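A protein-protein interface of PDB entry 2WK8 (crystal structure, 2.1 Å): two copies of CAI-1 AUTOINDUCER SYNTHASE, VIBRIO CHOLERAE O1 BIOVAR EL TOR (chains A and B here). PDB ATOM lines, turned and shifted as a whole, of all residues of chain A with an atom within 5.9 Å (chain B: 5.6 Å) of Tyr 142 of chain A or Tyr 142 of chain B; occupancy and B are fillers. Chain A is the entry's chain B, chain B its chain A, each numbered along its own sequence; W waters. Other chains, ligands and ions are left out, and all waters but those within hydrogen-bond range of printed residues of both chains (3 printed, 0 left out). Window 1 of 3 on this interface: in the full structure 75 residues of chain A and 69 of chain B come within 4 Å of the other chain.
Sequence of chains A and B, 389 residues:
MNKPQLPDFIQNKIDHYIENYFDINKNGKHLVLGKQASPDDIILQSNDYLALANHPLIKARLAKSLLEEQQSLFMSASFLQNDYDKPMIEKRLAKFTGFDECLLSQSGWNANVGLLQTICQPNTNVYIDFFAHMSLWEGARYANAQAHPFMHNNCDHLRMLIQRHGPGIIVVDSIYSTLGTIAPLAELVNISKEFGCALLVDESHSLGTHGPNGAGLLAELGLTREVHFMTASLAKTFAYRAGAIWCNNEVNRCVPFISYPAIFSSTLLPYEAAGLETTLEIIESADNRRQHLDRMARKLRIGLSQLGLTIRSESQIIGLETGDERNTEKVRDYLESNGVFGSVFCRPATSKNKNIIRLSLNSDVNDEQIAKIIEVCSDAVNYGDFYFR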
ATOM      1  N   TRP A 109      -2.274  -1.847   1.484  1.00  0.00           N
ATOM      2  CA  TRP A 109      -3.663  -1.696   1.885  1.00  0.00           C
ATOM      3  C   TRP A 109      -4.400  -3.049   1.856  1.00  0.00           C
ATOM      4  O   TRP A 109      -5.047  -3.436   2.837  1.00  0.00           O
ATOM      5  CB  TRP A 109      -4.394  -0.667   0.999  1.00  0.00           C
ATOM      6  CG  TRP A 109      -5.863  -0.592   1.305  1.00  0.00           C
ATOM      7  CD1 TRP A 109      -6.832  -1.513   0.956  1.00  0.00           C
ATOM      8  CD2 TRP A 109      -6.536   0.437   2.034  1.00  0.00           C
ATOM      9  NE1 TRP A 109      -8.058  -1.099   1.408  1.00  0.00           N
ATOM     10  CE2 TRP A 109      -7.914   0.082   2.084  1.00  0.00           C
ATOM     11  CE3 TRP A 109      -6.122   1.628   2.639  1.00  0.00           C
ATOM     12  CZ2 TRP A 109      -8.874   0.875   2.718  1.00  0.00           C
ATOM     13  CZ3 TRP A 109      -7.084   2.425   3.265  1.00  0.00           C
ATOM     14  CH2 TRP A 109      -8.446   2.038   3.302  1.00  0.00           C
ATOM     15  N   VAL A 113      -6.015  -5.287   5.044  1.00  0.00           N
ATOM     16  CA  VAL A 113      -7.439  -5.565   4.976  1.00  0.00           C
ATOM     17  C   VAL A 113      -7.742  -7.075   4.882  1.00  0.00           C
ATOM     18  O   VAL A 113      -8.681  -7.565   5.501  1.00  0.00           O
ATOM     19  CB  VAL A 113      -8.073  -4.802   3.785  1.00  0.00           C
ATOM     20  CG1 VAL A 113      -9.291  -5.502   3.303  1.00  0.00           C
ATOM     21  CG2 VAL A 113      -8.366  -3.347   4.180  1.00  0.00           C
ATOM     22  N   TRP A 137      -7.337   0.308  10.334  1.00  0.00           N
ATOM     23  CA  TRP A 137      -8.616   0.773  10.840  1.00  0.00           C
ATOM     24  C   TRP A 137      -9.733   0.195   9.980  1.00  0.00           C
ATOM     25  O   TRP A 137     -10.577  -0.570  10.463  1.00  0.00           O
ATOM     26  CB  TRP A 137      -8.678   2.301  10.871  1.00  0.00           C
ATOM     27  CG  TRP A 137      -7.911   2.917  12.020  1.00  0.00           C
ATOM     28  CD1 TRP A 137      -6.590   3.272  12.034  1.00  0.00           C
ATOM     29  CD2 TRP A 137      -8.423   3.239  13.322  1.00  0.00           C
ATOM     30  NE1 TRP A 137      -6.250   3.791  13.262  1.00  0.00           N
ATOM     31  CE2 TRP A 137      -7.356   3.787  14.067  1.00  0.00           C
ATOM     32  CE3 TRP A 137      -9.678   3.107  13.931  1.00  0.00           C
ATOM     33  CZ2 TRP A 137      -7.507   4.218  15.387  1.00  0.00           C
ATOM     34  CZ3 TRP A 137      -9.828   3.537  15.246  1.00  0.00           C
ATOM     35  CH2 TRP A 137      -8.744   4.084  15.961  1.00  0.00           C
ATOM     36  N   GLU A 138      -9.720   0.529   8.694  1.00  0.00           N
ATOM     37  CA  GLU A 138     -10.733   0.005   7.770  1.00  0.00           C
ATOM     38  C   GLU A 138     -10.807  -1.540   7.748  1.00  0.00           C
ATOM     39  O   GLU A 138     -11.884  -2.112   7.684  1.00  0.00           O
ATOM     40  CB  GLU A 138     -10.506   0.576   6.361  1.00  0.00           C
ATOM     41  CG  GLU A 138     -10.781   2.078   6.284  1.00  0.00           C
ATOM     42  CD  GLU A 138     -12.241   2.394   6.569  1.00  0.00           C
ATOM     43  OE1 GLU A 138     -13.059   2.335   5.629  1.00  0.00           O
ATOM     44  OE2 GLU A 138     -12.572   2.683   7.741  1.00  0.00           O
ATOM     45  N   GLY A 139      -9.665  -2.215   7.779  1.00  0.00           N
ATOM     46  CA  GLY A 139      -9.676  -3.664   7.785  1.00  0.00           C
ATOM     47  C   GLY A 139     -10.483  -4.219   8.954  1.00  0.00           C
ATOM     48  O   GLY A 139     -11.271  -5.157   8.783  1.00  0.00           O
ATOM     49  N   ALA A 140     -10.302  -3.633  10.142  1.00  0.00           N
ATOM     50  CA  ALA A 140     -10.999  -4.112  11.344  1.00  0.00           C
ATOM     51  C   ALA A 140     -12.488  -3.807  11.222  1.00  0.00           C
ATOM     52  O   ALA A 140     -13.340  -4.592  11.606  1.00  0.00           O
ATOM     53  CB  ALA A 140     -10.427  -3.472  12.601  1.00  0.00           C
ATOM     54  N   ARG A 141     -12.774  -2.661  10.639  1.00  0.00           N
ATOM     55  CA  ARG A 141     -14.125  -2.197  10.470  1.00  0.00           C
ATOM     56  C   ARG A 141     -14.878  -3.018   9.423  1.00  0.00           C
ATOM     57  O   ARG A 141     -16.041  -3.337   9.608  1.00  0.00           O
ATOM     58  CB  ARG A 141     -14.074  -0.721  10.076  1.00  0.00           C
ATOM     59  CG  ARG A 141     -15.415  -0.066   9.927  1.00  0.00           C
ATOM     60  CD  ARG A 141     -15.280   1.310   9.262  1.00  0.00           C
ATOM     61  NE  ARG A 141     -16.556   1.646   8.662  1.00  0.00           N
ATOM     62  CZ  ARG A 141     -16.773   1.889   7.375  1.00  0.00           C
ATOM     63  NH1 ARG A 141     -15.783   1.922   6.494  1.00  0.00           N
ATOM     64  NH2 ARG A 141     -18.008   2.153   6.986  1.00  0.00           N
ATOM     65  N   TYR A 142     -14.216  -3.357   8.319  1.00  0.00           N
ATOM     66  CA  TYR A 142     -14.834  -4.186   7.285  1.00  0.00           C
ATOM     67  C   TYR A 142     -15.241  -5.542   7.891  1.00  0.00           C
ATOM     68  O   TYR A 142     -16.247  -6.127   7.510  1.00  0.00           O
ATOM     69  CB  TYR A 142     -13.872  -4.422   6.097  1.00  0.00           C
ATOM     70  CG  TYR A 142     -13.487  -3.205   5.261  1.00  0.00           C
ATOM     71  CD1 TYR A 142     -14.142  -1.986   5.397  1.00  0.00           C
ATOM     72  CD2 TYR A 142     -12.482  -3.297   4.307  1.00  0.00           C
ATOM     73  CE1 TYR A 142     -13.781  -0.874   4.619  1.00  0.00           C
ATOM     74  CE2 TYR A 142     -12.121  -2.201   3.526  1.00  0.00           C
ATOM     75  CZ  TYR A 142     -12.772  -1.000   3.682  1.00  0.00           C
ATOM     76  OH  TYR A 142     -12.413   0.069   2.885  1.00  0.00           O
ATOM     77  N   ALA A 143     -14.436  -6.029   8.831  1.00  0.00           N
ATOM     78  CA  ALA A 143     -14.653  -7.316   9.492  1.00  0.00           C
ATOM     79  C   ALA A 143     -15.640  -7.215  10.634  1.00  0.00           C
ATOM     80  O   ALA A 143     -15.931  -8.216  11.303  1.00  0.00           O
ATOM     81  CB  ALA A 143     -13.331  -7.871  10.019  1.00  0.00           C
ATOM     82  N   ASN A 144     -16.129  -6.001  10.857  1.00  0.00           N
ATOM     83  CA  ASN A 144     -17.047  -5.713  11.948  1.00  0.00           C
ATOM     84  C   ASN A 144     -16.449  -6.014  13.322  1.00  0.00           C
ATOM     85  O   ASN A 144     -17.174  -6.321  14.270  1.00  0.00           O
ATOM     86  CB  ASN A 144     -18.376  -6.449  11.752  1.00  0.00           C
ATOM     87  CG  ASN A 144     -19.191  -5.883  10.595  1.00  0.00           C
ATOM     88  OD1 ASN A 144     -19.403  -6.558   9.591  1.00  0.00           O
ATOM     89  ND2 ASN A 144     -19.630  -4.630  10.724  1.00  0.00           N
ATOM     90  N   ALA A 145     -15.127  -5.904  13.419  1.00  0.00           N
ATOM     91  CA  ALA A 145     -14.421  -6.095  14.668  1.00  0.00           C
ATOM     92  C   ALA A 145     -14.766  -4.984  15.654  1.00  0.00           C
ATOM     93  O   ALA A 145     -15.327  -3.946  15.281  1.00  0.00           O
ATOM     94  CB  ALA A 145     -12.931  -6.137  14.420  1.00  0.00           C
ATOM     95  N   TYR A 260     -11.434 -10.728   0.718  1.00  0.00           N
ATOM     96  CA  TYR A 260     -12.099 -10.236  -0.476  1.00  0.00           C
ATOM     97  C   TYR A 260     -11.137  -9.676  -1.526  1.00  0.00           C
ATOM     98  O   TYR A 260     -11.245 -10.019  -2.696  1.00  0.00           O
ATOM     99  CB  TYR A 260     -13.222  -9.260  -0.123  1.00  0.00           C
ATOM    100  CG  TYR A 260     -14.469  -9.972   0.366  1.00  0.00           C
ATOM    101  CD1 TYR A 260     -14.454 -11.343   0.613  1.00  0.00           C
ATOM    102  CD2 TYR A 260     -15.649  -9.283   0.593  1.00  0.00           C
ATOM    103  CE1 TYR A 260     -15.585 -12.009   1.059  1.00  0.00           C
ATOM    104  CE2 TYR A 260     -16.788  -9.936   1.042  1.00  0.00           C
ATOM    105  CZ  TYR A 260     -16.751 -11.304   1.271  1.00  0.00           C
ATOM    106  OH  TYR A 260     -17.876 -11.968   1.721  1.00  0.00           O
ATOM    107  N   TRP B 109     -11.867  -3.277  -8.347  1.00  0.00           N
ATOM    108  CA  TRP B 109     -12.432  -3.306  -7.000  1.00  0.00           C
ATOM    109  C   TRP B 109     -12.342  -1.898  -6.395  1.00  0.00           C
ATOM    110  O   TRP B 109     -13.318  -1.365  -5.902  1.00  0.00           O
ATOM    111  CB  TRP B 109     -11.680  -4.320  -6.109  1.00  0.00           C
ATOM    112  CG  TRP B 109     -12.204  -4.409  -4.676  1.00  0.00           C
ATOM    113  CD1 TRP B 109     -11.916  -3.558  -3.642  1.00  0.00           C
ATOM    114  CD2 TRP B 109     -13.091  -5.401  -4.142  1.00  0.00           C
ATOM    115  NE1 TRP B 109     -12.568  -3.954  -2.501  1.00  0.00           N
ATOM    116  CE2 TRP B 109     -13.300  -5.085  -2.778  1.00  0.00           C
ATOM    117  CE3 TRP B 109     -13.728  -6.529  -4.681  1.00  0.00           C
ATOM    118  CZ2 TRP B 109     -14.131  -5.845  -1.951  1.00  0.00           C
ATOM    119  CZ3 TRP B 109     -14.555  -7.292  -3.857  1.00  0.00           C
ATOM    120  CH2 TRP B 109     -14.751  -6.942  -2.505  1.00  0.00           C
ATOM    121  N   VAL B 113     -15.356   0.663  -5.056  1.00  0.00           N
ATOM    122  CA  VAL B 113     -15.360   1.094  -3.665  1.00  0.00           C
ATOM    123  C   VAL B 113     -15.211   2.623  -3.576  1.00  0.00           C
ATOM    124  O   VAL B 113     -15.968   3.307  -2.867  1.00  0.00           O
ATOM    125  CB  VAL B 113     -14.228   0.368  -2.868  1.00  0.00           C
ATOM    126  CG1 VAL B 113     -13.850   1.134  -1.608  1.00  0.00           C
ATOM    127  CG2 VAL B 113     -14.655  -1.066  -2.535  1.00  0.00           C
ATOM    128  N   TRP B 137     -21.282  -4.471  -3.925  1.00  0.00           N
ATOM    129  CA  TRP B 137     -21.923  -4.724  -2.647  1.00  0.00           C
ATOM    130  C   TRP B 137     -21.071  -4.112  -1.552  1.00  0.00           C
ATOM    131  O   TRP B 137     -21.567  -3.342  -0.729  1.00  0.00           O
ATOM    132  CB  TRP B 137     -22.110  -6.227  -2.430  1.00  0.00           C
ATOM    133  CG  TRP B 137     -23.267  -6.770  -3.189  1.00  0.00           C
ATOM    134  CD1 TRP B 137     -23.271  -7.222  -4.483  1.00  0.00           C
ATOM    135  CD2 TRP B 137     -24.612  -6.897  -2.716  1.00  0.00           C
ATOM    136  NE1 TRP B 137     -24.535  -7.642  -4.834  1.00  0.00           N
ATOM    137  CE2 TRP B 137     -25.376  -7.443  -3.768  1.00  0.00           C
ATOM    138  CE3 TRP B 137     -25.242  -6.605  -1.502  1.00  0.00           C
ATOM    139  CZ2 TRP B 137     -26.741  -7.702  -3.643  1.00  0.00           C
ATOM    140  CZ3 TRP B 137     -26.593  -6.858  -1.377  1.00  0.00           C
ATOM    141  CH2 TRP B 137     -27.329  -7.412  -2.442  1.00  0.00           C
ATOM    142  N   GLU B 138     -19.780  -4.434  -1.559  1.00  0.00           N
ATOM    143  CA  GLU B 138     -18.908  -3.987  -0.482  1.00  0.00           C
ATOM    144  C   GLU B 138     -18.753  -2.465  -0.412  1.00  0.00           C
ATOM    145  O   GLU B 138     -18.746  -1.899   0.677  1.00  0.00           O
ATOM    146  CB  GLU B 138     -17.553  -4.697  -0.529  1.00  0.00           C
ATOM    147  CG  GLU B 138     -17.623  -6.156  -0.080  1.00  0.00           C
ATOM    148  CD  GLU B 138     -17.882  -6.287   1.409  1.00  0.00           C
ATOM    149  OE1 GLU B 138     -16.909  -6.251   2.182  1.00  0.00           O
ATOM    150  OE2 GLU B 138     -19.060  -6.415   1.795  1.00  0.00           O
ATOM    151  N   GLY B 139     -18.636  -1.798  -1.555  1.00  0.00           N
ATOM    152  CA  GLY B 139     -18.480  -0.348  -1.555  1.00  0.00           C
ATOM    153  C   GLY B 139     -19.642   0.352  -0.870  1.00  0.00           C
ATOM    154  O   GLY B 139     -19.474   1.274  -0.062  1.00  0.00           O
ATOM    155  N   ALA B 140     -20.841  -0.112  -1.186  1.00  0.00           N
ATOM    156  CA  ALA B 140     -22.050   0.463  -0.614  1.00  0.00           C
ATOM    157  C   ALA B 140     -22.072   0.193   0.879  1.00  0.00           C
ATOM    158  O   ALA B 140     -22.440   1.048   1.670  1.00  0.00           O
ATOM    159  CB  ALA B 140     -23.300  -0.124  -1.304  1.00  0.00           C
ATOM    160  N   ARG B 141     -21.666  -1.011   1.257  1.00  0.00           N
ATOM    161  CA  ARG B 141     -21.721  -1.416   2.638  1.00  0.00           C
ATOM    162  C   ARG B 141     -20.710  -0.612   3.428  1.00  0.00           C
ATOM    163  O   ARG B 141     -20.998  -0.138   4.530  1.00  0.00           O
ATOM    164  CB  ARG B 141     -21.460  -2.921   2.749  1.00  0.00           C
ATOM    165  CG  ARG B 141     -21.178  -3.394   4.152  1.00  0.00           C
ATOM    166  CD  ARG B 141     -20.703  -4.841   4.142  1.00  0.00           C
ATOM    167  NE  ARG B 141     -20.192  -5.183   5.457  1.00  0.00           N
ATOM    168  CZ  ARG B 141     -18.929  -5.474   5.728  1.00  0.00           C
ATOM    169  NH1 ARG B 141     -18.016  -5.514   4.771  1.00  0.00           N
ATOM    170  NH2 ARG B 141     -18.589  -5.748   6.971  1.00  0.00           N
ATOM    171  N   TYR B 142     -19.526  -0.446   2.845  1.00  0.00           N
ATOM    172  CA  TYR B 142     -18.472   0.347   3.457  1.00  0.00           C
ATOM    173  C   TYR B 142     -18.943   1.783   3.661  1.00  0.00           C
ATOM    174  O   TYR B 142     -18.507   2.464   4.586  1.00  0.00           O
ATOM    175  CB  TYR B 142     -17.201   0.342   2.600  1.00  0.00           C
ATOM    176  CG  TYR B 142     -16.553  -1.019   2.392  1.00  0.00           C
ATOM    177  CD1 TYR B 142     -16.910  -2.130   3.171  1.00  0.00           C
ATOM    178  CD2 TYR B 142     -15.555  -1.184   1.434  1.00  0.00           C
ATOM    179  CE1 TYR B 142     -16.296  -3.400   2.962  1.00  0.00           C
ATOM    180  CE2 TYR B 142     -14.935  -2.426   1.230  1.00  0.00           C
ATOM    181  CZ  TYR B 142     -15.300  -3.520   1.996  1.00  0.00           C
ATOM    182  OH  TYR B 142     -14.685  -4.734   1.753  1.00  0.00           O
ATOM    183  N   ALA B 143     -19.836   2.237   2.788  1.00  0.00           N
ATOM    184  CA  ALA B 143     -20.358   3.593   2.855  1.00  0.00           C
ATOM    185  C   ALA B 143     -21.586   3.662   3.763  1.00  0.00           C
ATOM    186  O   ALA B 143     -22.181   4.722   3.940  1.00  0.00           O
ATOM    187  CB  ALA B 143     -20.704   4.090   1.440  1.00  0.00           C
ATOM    188  N   ASN B 144     -21.967   2.521   4.327  1.00  0.00           N
ATOM    189  CA  ASN B 144     -23.153   2.448   5.174  1.00  0.00           C
ATOM    190  C   ASN B 144     -24.414   2.913   4.463  1.00  0.00           C
ATOM    191  O   ASN B 144     -25.289   3.562   5.054  1.00  0.00           O
ATOM    192  CB  ASN B 144     -22.942   3.245   6.455  1.00  0.00           C
ATOM    193  CG  ASN B 144     -21.984   2.566   7.391  1.00  0.00           C
ATOM    194  OD1 ASN B 144     -20.896   3.065   7.635  1.00  0.00           O
ATOM    195  ND2 ASN B 144     -22.367   1.391   7.893  1.00  0.00           N
ATOM    196  N   TYR B 260     -10.953   6.172   0.149  1.00  0.00           N
ATOM    197  CA  TYR B 260      -9.882   5.667   0.999  1.00  0.00           C
ATOM    198  C   TYR B 260      -8.817   4.877   0.208  1.00  0.00           C
ATOM    199  O   TYR B 260      -7.619   5.114   0.379  1.00  0.00           O
ATOM    200  CB  TYR B 260     -10.455   4.859   2.164  1.00  0.00           C
ATOM    201  CG  TYR B 260     -10.975   5.699   3.327  1.00  0.00           C
ATOM    202  CD1 TYR B 260     -11.047   7.089   3.235  1.00  0.00           C
ATOM    203  CD2 TYR B 260     -11.396   5.097   4.514  1.00  0.00           C
ATOM    204  CE1 TYR B 260     -11.513   7.860   4.284  1.00  0.00           C
ATOM    205  CE2 TYR B 260     -11.872   5.864   5.582  1.00  0.00           C
ATOM    206  CZ  TYR B 260     -11.927   7.243   5.461  1.00  0.00           C
ATOM    207  OH  TYR B 260     -12.388   8.011   6.510  1.00  0.00           O
ATOM    208  N   PRO B 261      -9.247   3.956  -0.670  1.00  0.00           N
ATOM    209  CA  PRO B 261      -8.262   3.322  -1.555  1.00  0.00           C
ATOM    210  C   PRO B 261      -7.508   4.322  -2.422  1.00  0.00           C
ATOM    211  O   PRO B 261      -6.328   4.131  -2.620  1.00  0.00           O
ATOM    212  CB  PRO B 261      -9.113   2.405  -2.426  1.00  0.00           C
ATOM    213  CG  PRO B 261     -10.278   2.035  -1.536  1.00  0.00           C
ATOM    214  CD  PRO B 261     -10.572   3.311  -0.767  1.00  0.00           C
HETATM  215  O   HOH W   1     -19.353   0.186   9.091  1.00  0.00           O
HETATM  216  O   HOH W   2     -21.234  -3.199   8.024  1.00  0.00           O
HETATM  217  O   HOH W   3     -21.536  -6.098   7.964  1.00  0.00           O
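NH1 of Arg 141 of chain B is in salt-bridge range of OE1 of Glu 138 of chain B.
The side-chain carboxylate of Glu 138 of chain B is in hydrogen-bond range of the side-chain hydroxyl of Tyr 142 of chain B (2.7 Å).
OE1 of Glu 138 of chain A lies within salt-bridge range of NH1 of Arg 141 of chain A (2.9 Å).
NH2 of Arg 141 of chain B is in hydrogen-bond range of O of Tyr 142 of chain A, 2.4 Å away.
NH2 of Arg 141 of chain B lies within hydrogen-bond range of OD1 of Asn 144 of chain A.
The backbone carbonyl oxygen (O) of Tyr 142 of chain B is in hydrogen-bond range of the guanidinium group (NH2) of Arg 141 of chain A.
The side-chain amide oxygen (OD1) of Asn 144 of chain B sits at hydrogen-bond distance from the guanidinium group (NH2) of Arg 141 of chain A.
Among the printed residues, pairs that only touch across the chains: Glu 138 of chain A with Tyr 260 of chain B (3.4 Å), Tyr 142 of chain A with Tyr 142 of chain B (3.5 Å), Trp 109 of chain A with Tyr 260 of chain B (3.6 Å), Tyr 260 of chain A with Glu 138 of chain B (3.6 Å) and Tyr 260 of chain A with Trp 109 of chain B (3.7 Å).
Water W3 lies within hydrogen-bond range of the side-chain amide oxygen of Asn 144 of chain A (2.7 Å) and the guanidinium group of Arg 141 of chain B (3.0 Å).
Water W1 bridges the guanidinium group of Arg 141 of chain A (3.2 Å) and the side-chain amide nitrogen of Asn 144 of chain B (3.5 Å).
Water W2 bridges NE of Arg 141 of chain B (3.4 Å) and ND2 of Asn 144 of chain A (3.5 Å).
Hydrophobic or aromatic side chains of chain B within 4 Å of the printed part of chain A: Trp 109, Tyr 142 and Tyr 260.
Of the 12 printed residues of chain A, 6 touch a printed residue of chain B.
Printed residues of chain A that touch a printed residue of chain B: Trp 109, Glu 138, Arg 141, Tyr 142, Asn 144 and Tyr 260.
Hydrophobic or aromatic side chains of chain A within 4 Å of the printed part of chain B: Trp 109, Tyr 142 and Tyr 260.
Among the printed residues, no Asp or Glu carboxylate lies within 4 Å of a Lys or Arg side-chain nitrogen of the other chain.
Tyr 142 of chain A touches just these residues of chain B: Arg 141 and Tyr 142.
Tyr 142 of chain B touches just these residues of chain A: Arg 141 (2.5 Å) and Tyr 142 (3.5 Å).
Printed residues of chain B within 4 Å of Asn 144 of chain A: Arg 141.
Printed residues of chain B within 4 Å of Tyr 260 of chain A: Trp 109 and Glu 138.
Of the printed residues of chain B, Trp 109 of chain A touches Tyr 260.
Of the printed residues of chain A, Asn 144 of chain B touches Arg 141.
Gly 139 of chain B touches none of the printed residues of chain A.
The nearest printed residue of chain B that does not touch Arg 141 of chain A is Arg 141 of chain B (4.4 Å).
Trp 109 of chain A touches Tyr 260 of chain B, and with the chains exchanged Tyr 260 of chain A touches Trp 109 of chain B.
Arg 141 of chain A touches Tyr 142 of chain B, and with the chains exchanged Tyr 142 of chain A touches Arg 141 of chain B.
Arg 141 of chain A touches Asn 144 of chain B, and with the chains exchanged Asn 144 of chain A touches Arg 141 of chain B.
Tyr 142 of chain A touches its own counterpart, Tyr 142 of chain B.
11 positions are printed for both chains.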
